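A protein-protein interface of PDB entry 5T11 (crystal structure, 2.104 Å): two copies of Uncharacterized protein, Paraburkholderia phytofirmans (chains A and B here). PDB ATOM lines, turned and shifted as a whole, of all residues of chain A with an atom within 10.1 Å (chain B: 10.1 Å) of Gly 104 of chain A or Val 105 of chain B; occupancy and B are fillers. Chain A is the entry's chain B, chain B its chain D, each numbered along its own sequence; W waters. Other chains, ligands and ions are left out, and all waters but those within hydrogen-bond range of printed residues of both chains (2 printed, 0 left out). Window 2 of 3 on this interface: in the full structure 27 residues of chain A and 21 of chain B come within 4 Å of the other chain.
Among the printed residues, merely in contact across the chains: Arg 100 of chain A with Tyr 101 of chain B, Lys 102 of chain A with Tyr 101 of chain B, Lys 102 of chain A with Arg 138 of chain B, Thr 103 of chain A with Gly 104 of chain B, Gly 104 of chain A with Val 105 of chain B and Trp 136 of chain A with Arg 138 of chain B.
Water W1 bridges the side-chain carboxylate of Asp 106 of chain B (2.7 Å) and the side-chain carboxylate of Glu 108 of chain A (2.8 Å). Water W2 bridges O of Thr 103 of chain A (2.9 Å) and N of Asp 106 of chain B (2.9 Å).
The side-chain amino group (NZ) of Lys 102 of chain A lies within hydrogen-bond range of the backbone carbonyl oxygen (O) of Ser 137 of chain B, at 2.8 Å. The side-chain carboxylate (OE2) of Glu 108 of chain A lies within salt-bridge range of the guanidinium group (NE) of Arg 138 of chain B (3.0 Å). OG of Ser 137 of chain A is in hydrogen-bond range of NH2 of Arg 138 of chain B, at 3.1 Å.
Lys 102 of chain A touches Tyr 101 of chain B, but with the chains exchanged Tyr 101 of chain A does not touch Lys 102 of chain B (10.9 Å). Lys 102 of chain A touches Arg 138 of chain B, but with the chains exchanged Arg 138 of chain A does not touch Lys 102 of chain B (18.7 Å). Thr 103 of chain A touches Gly 104 of chain B, but with the chains exchanged Gly 104 of chain A does not touch Thr 103 of chain B (9.5 Å). Gly 104 of chain A touches Val 105 of chain B, but with the chains exchanged Val 105 of chain A does not touch Gly 104 of chain B (8.9 Å). Of the 9 pairs that touch across the chains among the printed residues, none has its exchanged pair printed and touching as well.
Hydrophobic or aromatic side chains of chain A within 4 Å of the printed part of chain B: Trp 136.
The side-chain amino group (NZ) of Lys 102 of chain A is in salt-bridge range of the side-chain carboxylate (OE2) of Glu 108 of chain A (2.8 Å). O of Asp 106 of chain A sits close to OG of Ser 137 of chain A, at 3.3 Å.
Of chain B, only Gly 104 comes within 4 Å of Thr 103 of chain A. Gly 104 of chain A touches just one residue of chain B: Val 105 (3.9 Å). No residue of chain B comes within 4 Å of Val 105 of chain A. Gly 107 of chain A touches none of the printed residues of chain B. Val 105 of chain B touches just one residue of chain A: Gly 104 (3.9 Å). No residue of chain A comes within 4 Å of Asp 106 of chain B. Printed residues of chain A within 4 Å of Ser 137 of chain B: Lys 102 (2.8 Å). Of the printed residues of chain A, Arg 138 of chain B touches Lys 102 (3.5 Å), Glu 108 (3.0 Å), Trp 136 (3.6 Å) and Ser 137 (3.1 Å). The nearest residue of chain B that does not touch Gly 104 of chain A is Asp 106 of chain B (6.6 Å). The nearest residue of chain A that does not touch Val 105 of chain B is Thr 103 of chain A (4.2 Å).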
ATOM      1  N   ARG A 100      -5.820 -28.432  -3.088  1.00  0.00           N
ATOM      2  CA  ARG A 100      -5.187 -28.648  -1.787  1.00  0.00           C
ATOM      3  C   ARG A 100      -6.052 -29.602  -0.984  1.00  0.00           C
ATOM      4  O   ARG A 100      -7.204 -29.875  -1.340  1.00  0.00           O
ATOM      5  CB  ARG A 100      -5.014 -27.325  -1.028  1.00  0.00           C
ATOM      6  CG  ARG A 100      -6.367 -26.644  -0.702  1.00  0.00           C
ATOM      7  CD  ARG A 100      -6.217 -25.432   0.221  1.00  0.00           C
ATOM      8  NE  ARG A 100      -5.655 -25.815   1.525  1.00  0.00           N
ATOM      9  CZ  ARG A 100      -5.567 -24.998   2.569  1.00  0.00           C
ATOM     10  NH1 ARG A 100      -5.996 -23.737   2.480  1.00  0.00           N
ATOM     11  NH2 ARG A 100      -5.053 -25.439   3.704  1.00  0.00           N
ATOM     12  N   TYR A 101      -5.485 -30.111   0.112  1.00  0.00           N
ATOM     13  CA  TYR A 101      -6.312 -30.633   1.194  1.00  0.00           C
ATOM     14  C   TYR A 101      -6.624 -29.475   2.124  1.00  0.00           C
ATOM     15  O   TYR A 101      -5.762 -28.631   2.388  1.00  0.00           O
ATOM     16  CB  TYR A 101      -5.624 -31.762   1.976  1.00  0.00           C
ATOM     17  CG  TYR A 101      -5.339 -33.008   1.151  1.00  0.00           C
ATOM     18  CD1 TYR A 101      -6.321 -33.981   0.970  1.00  0.00           C
ATOM     19  CD2 TYR A 101      -4.090 -33.209   0.542  1.00  0.00           C
ATOM     20  CE1 TYR A 101      -6.084 -35.124   0.212  1.00  0.00           C
ATOM     21  CE2 TYR A 101      -3.841 -34.366  -0.230  1.00  0.00           C
ATOM     22  CZ  TYR A 101      -4.852 -35.314  -0.388  1.00  0.00           C
ATOM     23  OH  TYR A 101      -4.650 -36.457  -1.142  1.00  0.00           O
ATOM     24  N   LYS A 102      -7.871 -29.407   2.588  1.00  0.00           N
ATOM     25  CA  LYS A 102      -8.166 -28.447   3.635  1.00  0.00           C
ATOM     26  C   LYS A 102      -7.379 -28.832   4.888  1.00  0.00           C
ATOM     27  O   LYS A 102      -6.863 -29.948   5.013  1.00  0.00           O
ATOM     28  CB  LYS A 102      -9.679 -28.375   3.908  1.00  0.00           C
ATOM     29  CG  LYS A 102     -10.460 -27.685   2.759  1.00  0.00           C
ATOM     30  CD  LYS A 102     -11.987 -27.962   2.782  1.00  0.00           C
ATOM     31  CE  LYS A 102     -12.641 -27.590   4.085  1.00  0.00           C
ATOM     32  NZ  LYS A 102     -14.160 -27.578   3.934  1.00  0.00           N
ATOM     33  N   THR A 103      -7.271 -27.884   5.808  1.00  0.00           N
ATOM     34  CA  THR A 103      -6.332 -28.011   6.911  1.00  0.00           C
ATOM     35  C   THR A 103      -6.836 -29.019   7.939  1.00  0.00           C
ATOM     36  O   THR A 103      -8.041 -29.214   8.124  1.00  0.00           O
ATOM     37  CB  THR A 103      -6.098 -26.641   7.557  1.00  0.00           C
ATOM     38  OG1 THR A 103      -4.865 -26.657   8.282  1.00  0.00           O
ATOM     39  CG2 THR A 103      -7.233 -26.285   8.519  1.00  0.00           C
ATOM     40  N   GLY A 104      -5.895 -29.686   8.589  1.00  0.00           N
ATOM     41  CA  GLY A 104      -6.217 -30.616   9.649  1.00  0.00           C
ATOM     42  C   GLY A 104      -6.114 -32.069   9.201  1.00  0.00           C
ATOM     43  O   GLY A 104      -6.169 -32.402   8.010  1.00  0.00           O
ATOM     44  N   VAL A 105      -5.923 -32.939  10.189  1.00  0.00           N
ATOM     45  CA  VAL A 105      -6.067 -34.370   9.994  1.00  0.00           C
ATOM     46  C   VAL A 105      -7.423 -34.644   9.358  1.00  0.00           C
ATOM     47  O   VAL A 105      -8.446 -34.108   9.793  1.00  0.00           O
ATOM     48  CB  VAL A 105      -5.911 -35.088  11.347  1.00  0.00           C
ATOM     49  CG1 VAL A 105      -6.317 -36.536  11.225  1.00  0.00           C
ATOM     50  CG2 VAL A 105      -4.478 -34.941  11.860  1.00  0.00           C
ATOM     51  N   ASP A 106      -7.434 -35.475   8.320  1.00  0.00           N
ATOM     52  CA  ASP A 106      -8.655 -35.795   7.577  1.00  0.00           C
ATOM     53  C   ASP A 106      -9.278 -34.571   6.896  1.00  0.00           C
ATOM     54  O   ASP A 106     -10.449 -34.603   6.518  1.00  0.00           O
ATOM     55  CB  ASP A 106      -9.699 -36.486   8.467  1.00  0.00           C
ATOM     56  CG  ASP A 106      -9.364 -37.938   8.731  1.00  0.00           C
ATOM     57  OD1 ASP A 106      -8.823 -38.596   7.812  1.00  0.00           O
ATOM     58  OD2 ASP A 106      -9.637 -38.420   9.850  1.00  0.00           O
ATOM     59  N   GLY A 107      -8.516 -33.497   6.704  1.00  0.00           N
ATOM     60  CA  GLY A 107      -8.978 -32.417   5.856  1.00  0.00           C
ATOM     61  C   GLY A 107      -9.202 -32.922   4.441  1.00  0.00           C
ATOM     62  O   GLY A 107      -8.343 -33.618   3.877  1.00  0.00           O
ATOM     63  N   GLU A 108     -10.361 -32.560   3.851  1.00  0.00           N
ATOM     64  CA  GLU A 108     -10.816 -33.085   2.575  1.00  0.00           C
ATOM     65  C   GLU A 108     -10.113 -32.404   1.396  1.00  0.00           C
ATOM     66  O   GLU A 108      -9.751 -31.225   1.471  1.00  0.00           O
ATOM     67  CB  GLU A 108     -12.333 -32.916   2.440  1.00  0.00           C
ATOM     68  CG  GLU A 108     -12.840 -31.490   2.490  1.00  0.00           C
ATOM     69  CD  GLU A 108     -13.286 -31.063   3.892  1.00  0.00           C
ATOM     70  OE1 GLU A 108     -12.614 -31.427   4.885  1.00  0.00           O
ATOM     71  OE2 GLU A 108     -14.320 -30.361   3.998  1.00  0.00           O
ATOM     72  N   PRO A 109      -9.907 -33.131   0.299  1.00  0.00           N
ATOM     73  CA  PRO A 109      -9.373 -32.502  -0.919  1.00  0.00           C
ATOM     74  C   PRO A 109     -10.393 -31.587  -1.575  1.00  0.00           C
ATOM     75  O   PRO A 109     -11.597 -31.847  -1.560  1.00  0.00           O
ATOM     76  CB  PRO A 109      -9.058 -33.701  -1.829  1.00  0.00           C
ATOM     77  CG  PRO A 109     -10.015 -34.787  -1.371  1.00  0.00           C
ATOM     78  CD  PRO A 109     -10.118 -34.582   0.140  1.00  0.00           C
ATOM     79  N   TRP A 136     -14.554 -36.315   0.254  1.00  0.00           N
ATOM     80  CA  TRP A 136     -14.695 -36.493   1.697  1.00  0.00           C
ATOM     81  C   TRP A 136     -13.302 -36.667   2.309  1.00  0.00           C
ATOM     82  O   TRP A 136     -12.289 -36.670   1.612  1.00  0.00           O
ATOM     83  CB  TRP A 136     -15.623 -37.659   2.076  1.00  0.00           C
ATOM     84  CG  TRP A 136     -15.891 -37.761   3.653  1.00  0.00           C
ATOM     85  CD1 TRP A 136     -16.662 -36.917   4.441  1.00  0.00           C
ATOM     86  CD2 TRP A 136     -15.347 -38.737   4.560  1.00  0.00           C
ATOM     87  NE1 TRP A 136     -16.634 -37.331   5.758  1.00  0.00           N
ATOM     88  CE2 TRP A 136     -15.838 -38.445   5.852  1.00  0.00           C
ATOM     89  CE3 TRP A 136     -14.499 -39.835   4.403  1.00  0.00           C
ATOM     90  CZ2 TRP A 136     -15.487 -39.206   6.969  1.00  0.00           C
ATOM     91  CZ3 TRP A 136     -14.169 -40.591   5.514  1.00  0.00           C
ATOM     92  CH2 TRP A 136     -14.664 -40.275   6.777  1.00  0.00           C
ATOM     93  N   SER A 137     -13.259 -36.801   3.632  1.00  0.00           N
ATOM     94  CA  SER A 137     -12.001 -36.912   4.355  1.00  0.00           C
ATOM     95  C   SER A 137     -11.136 -38.052   3.841  1.00  0.00           C
ATOM     96  O   SER A 137      -9.904 -37.982   3.933  1.00  0.00           O
ATOM     97  CB  SER A 137     -12.290 -37.105   5.837  1.00  0.00           C
ATOM     98  OG  SER A 137     -13.301 -36.218   6.232  1.00  0.00           O
ATOM     99  N   ARG A 138     -11.749 -39.108   3.310  1.00  0.00           N
ATOM    100  CA  ARG A 138     -10.997 -40.286   2.902  1.00  0.00           C
ATOM    101  C   ARG A 138     -10.484 -40.213   1.471  1.00  0.00           C
ATOM    102  O   ARG A 138      -9.716 -41.090   1.069  1.00  0.00           O
ATOM    103  CB  ARG A 138     -11.854 -41.549   3.046  1.00  0.00           C
ATOM    104  CG  ARG A 138     -12.832 -41.723   1.895  1.00  0.00           C
ATOM    105  CD  ARG A 138     -13.486 -43.097   1.883  1.00  0.00           C
ATOM    106  NE  ARG A 138     -14.351 -43.307   3.038  1.00  0.00           N
ATOM    107  CZ  ARG A 138     -15.489 -42.653   3.234  1.00  0.00           C
ATOM    108  NH1 ARG A 138     -16.228 -42.903   4.309  1.00  0.00           N
ATOM    109  NH2 ARG A 138     -15.876 -41.729   2.359  1.00  0.00           N
ATOM    110  N   ARG B 100     -10.960 -16.809   1.763  1.00  0.00           N
ATOM    111  CA  ARG B 100     -10.165 -17.647   2.651  1.00  0.00           C
ATOM    112  C   ARG B 100     -11.070 -18.686   3.283  1.00  0.00           C
ATOM    113  O   ARG B 100     -12.300 -18.618   3.184  1.00  0.00           O
ATOM    114  CB  ARG B 100      -9.492 -16.814   3.756  1.00  0.00           C
ATOM    115  CG  ARG B 100     -10.529 -16.055   4.653  1.00  0.00           C
ATOM    116  CD  ARG B 100      -9.890 -15.328   5.840  1.00  0.00           C
ATOM    117  NE  ARG B 100      -9.284 -16.263   6.786  1.00  0.00           N
ATOM    118  CZ  ARG B 100      -8.766 -15.920   7.964  1.00  0.00           C
ATOM    119  NH1 ARG B 100      -8.767 -14.653   8.365  1.00  0.00           N
ATOM    120  NH2 ARG B 100      -8.241 -16.846   8.746  1.00  0.00           N
ATOM    121  N   TYR B 101     -10.441 -19.623   3.983  1.00  0.00           N
ATOM    122  CA  TYR B 101     -11.132 -20.428   4.976  1.00  0.00           C
ATOM    123  C   TYR B 101     -10.941 -19.739   6.314  1.00  0.00           C
ATOM    124  O   TYR B 101      -9.831 -19.306   6.625  1.00  0.00           O
ATOM    125  CB  TYR B 101     -10.573 -21.853   5.052  1.00  0.00           C
ATOM    126  CG  TYR B 101     -10.773 -22.656   3.794  1.00  0.00           C
ATOM    127  CD1 TYR B 101     -11.980 -23.303   3.561  1.00  0.00           C
ATOM    128  CD2 TYR B 101      -9.763 -22.763   2.839  1.00  0.00           C
ATOM    129  CE1 TYR B 101     -12.192 -24.038   2.422  1.00  0.00           C
ATOM    130  CE2 TYR B 101      -9.969 -23.511   1.651  1.00  0.00           C
ATOM    131  CZ  TYR B 101     -11.193 -24.146   1.468  1.00  0.00           C
ATOM    132  OH  TYR B 101     -11.468 -24.889   0.342  1.00  0.00           O
ATOM    133  N   LYS B 102     -12.013 -19.624   7.096  1.00  0.00           N
ATOM    134  CA  LYS B 102     -11.823 -19.136   8.453  1.00  0.00           C
ATOM    135  C   LYS B 102     -10.901 -20.099   9.198  1.00  0.00           C
ATOM    136  O   LYS B 102     -10.686 -21.245   8.784  1.00  0.00           O
ATOM    137  CB  LYS B 102     -13.174 -18.963   9.163  1.00  0.00           C
ATOM    138  CG  LYS B 102     -13.941 -17.720   8.674  1.00  0.00           C
ATOM    139  CD  LYS B 102     -15.443 -17.742   8.981  1.00  0.00           C
ATOM    140  CE  LYS B 102     -15.735 -17.655  10.469  1.00  0.00           C
ATOM    141  NZ  LYS B 102     -17.206 -17.458  10.704  1.00  0.00           N
ATOM    142  N   THR B 103     -10.325 -19.616  10.285  1.00  0.00           N
ATOM    143  CA  THR B 103      -9.222 -20.319  10.915  1.00  0.00           C
ATOM    144  C   THR B 103      -9.733 -21.555  11.641  1.00  0.00           C
ATOM    145  O   THR B 103     -10.881 -21.613  12.085  1.00  0.00           O
ATOM    146  CB  THR B 103      -8.473 -19.387  11.881  1.00  0.00           C
ATOM    147  OG1 THR B 103      -7.197 -19.945  12.200  1.00  0.00           O
ATOM    148  CG2 THR B 103      -9.251 -19.191  13.183  1.00  0.00           C
ATOM    149  N   GLY B 104      -8.874 -22.561  11.729  1.00  0.00           N
ATOM    150  CA  GLY B 104      -9.163 -23.773  12.465  1.00  0.00           C
ATOM    151  C   GLY B 104      -9.592 -24.912  11.556  1.00  0.00           C
ATOM    152  O   GLY B 104      -9.981 -24.722  10.399  1.00  0.00           O
ATOM    153  N   VAL B 105      -9.517 -26.124  12.107  1.00  0.00           N
ATOM    154  CA  VAL B 105     -10.046 -27.298  11.430  1.00  0.00           C
ATOM    155  C   VAL B 105     -11.539 -27.108  11.186  1.00  0.00           C
ATOM    156  O   VAL B 105     -12.270 -26.631  12.057  1.00  0.00           O
ATOM    157  CB  VAL B 105      -9.755 -28.546  12.281  1.00  0.00           C
ATOM    158  CG1 VAL B 105     -10.403 -29.771  11.670  1.00  0.00           C
ATOM    159  CG2 VAL B 105      -8.246 -28.742  12.418  1.00  0.00           C
ATOM    160  N   ASP B 106     -12.006 -27.457   9.989  1.00  0.00           N
ATOM    161  CA  ASP B 106     -13.396 -27.196   9.599  1.00  0.00           C
ATOM    162  C   ASP B 106     -13.752 -25.712   9.634  1.00  0.00           C
ATOM    163  O   ASP B 106     -14.930 -25.365   9.708  1.00  0.00           O
ATOM    164  CB  ASP B 106     -14.401 -27.966  10.468  1.00  0.00           C
ATOM    165  CG  ASP B 106     -14.298 -29.463  10.297  1.00  0.00           C
ATOM    166  OD1 ASP B 106     -13.979 -29.912   9.175  1.00  0.00           O
ATOM    167  OD2 ASP B 106     -14.538 -30.187  11.288  1.00  0.00           O
ATOM    168  N   GLY B 107     -12.773 -24.813   9.580  1.00  0.00           N
ATOM    169  CA  GLY B 107     -13.095 -23.425   9.286  1.00  0.00           C
ATOM    170  C   GLY B 107     -13.775 -23.272   7.931  1.00  0.00           C
ATOM    171  O   GLY B 107     -13.269 -23.767   6.919  1.00  0.00           O
ATOM    172  N   GLU B 108     -14.924 -22.585   7.895  1.00  0.00           N
ATOM    173  CA  GLU B 108     -15.741 -22.488   6.691  1.00  0.00           C
ATOM    174  C   GLU B 108     -15.142 -21.489   5.696  1.00  0.00           C
ATOM    175  O   GLU B 108     -14.505 -20.510   6.090  1.00  0.00           O
ATOM    176  CB  GLU B 108     -17.163 -22.057   7.049  1.00  0.00           C
ATOM    177  CG  GLU B 108     -17.250 -20.699   7.744  1.00  0.00           C
ATOM    178  CD  GLU B 108     -17.252 -20.783   9.273  1.00  0.00           C
ATOM    179  OE1 GLU B 108     -16.456 -21.575   9.842  1.00  0.00           O
ATOM    180  OE2 GLU B 108     -18.057 -20.042   9.905  1.00  0.00           O
ATOM    181  N   PRO B 109     -15.340 -21.708   4.400  1.00  0.00           N
ATOM    182  CA  PRO B 109     -14.899 -20.711   3.419  1.00  0.00           C
ATOM    183  C   PRO B 109     -15.780 -19.471   3.436  1.00  0.00           C
ATOM    184  O   PRO B 109     -16.991 -19.535   3.659  1.00  0.00           O
ATOM    185  CB  PRO B 109     -15.026 -21.453   2.087  1.00  0.00           C
ATOM    186  CG  PRO B 109     -16.144 -22.428   2.310  1.00  0.00           C
ATOM    187  CD  PRO B 109     -16.029 -22.849   3.763  1.00  0.00           C
ATOM    188  N   TRP B 136     -20.696 -23.617   4.483  1.00  0.00           N
ATOM    189  CA  TRP B 136     -20.650 -24.354   5.729  1.00  0.00           C
ATOM    190  C   TRP B 136     -19.291 -25.036   5.823  1.00  0.00           C
ATOM    191  O   TRP B 136     -18.437 -24.897   4.939  1.00  0.00           O
ATOM    192  CB  TRP B 136     -21.863 -25.281   5.847  1.00  0.00           C
ATOM    193  CG  TRP B 136     -21.702 -26.761   5.622  1.00  0.00           C
ATOM    194  CD1 TRP B 136     -21.679 -27.413   4.418  1.00  0.00           C
ATOM    195  CD2 TRP B 136     -21.641 -27.783   6.633  1.00  0.00           C
ATOM    196  NE1 TRP B 136     -21.572 -28.772   4.617  1.00  0.00           N
ATOM    197  CE2 TRP B 136     -21.547 -29.025   5.965  1.00  0.00           C
ATOM    198  CE3 TRP B 136     -21.640 -27.767   8.038  1.00  0.00           C
ATOM    199  CZ2 TRP B 136     -21.450 -30.235   6.650  1.00  0.00           C
ATOM    200  CZ3 TRP B 136     -21.539 -28.969   8.715  1.00  0.00           C
ATOM    201  CH2 TRP B 136     -21.443 -30.187   8.022  1.00  0.00           C
ATOM    202  N   SER B 137     -19.068 -25.751   6.925  1.00  0.00           N
ATOM    203  CA  SER B 137     -17.716 -26.171   7.269  1.00  0.00           C
ATOM    204  C   SER B 137     -17.123 -27.147   6.252  1.00  0.00           C
ATOM    205  O   SER B 137     -15.898 -27.191   6.083  1.00  0.00           O
ATOM    206  CB  SER B 137     -17.727 -26.793   8.652  1.00  0.00           C
ATOM    207  OG  SER B 137     -18.624 -27.884   8.662  1.00  0.00           O
ATOM    208  N   ARG B 138     -17.956 -27.940   5.579  1.00  0.00           N
ATOM    209  CA  ARG B 138     -17.451 -28.978   4.690  1.00  0.00           C
ATOM    210  C   ARG B 138     -17.466 -28.560   3.222  1.00  0.00           C
ATOM    211  O   ARG B 138     -17.431 -29.425   2.342  1.00  0.00           O
ATOM    212  CB  ARG B 138     -18.240 -30.272   4.887  1.00  0.00           C
ATOM    213  CG  ARG B 138     -18.184 -30.826   6.317  1.00  0.00           C
ATOM    214  CD  ARG B 138     -16.766 -30.904   6.881  1.00  0.00           C
ATOM    215  NE  ARG B 138     -15.911 -31.799   6.106  1.00  0.00           N
ATOM    216  CZ  ARG B 138     -15.960 -33.128   6.169  1.00  0.00           C
ATOM    217  NH1 ARG B 138     -16.832 -33.735   6.970  1.00  0.00           N
ATOM    218  NH2 ARG B 138     -15.139 -33.855   5.420  1.00  0.00           N
HETATM  219  O   HOH W   1     -12.487 -29.481   6.938  1.00  0.00           O
HETATM  220  O   HOH W   2     -10.536 -27.925   7.575  1.00  0.00           O
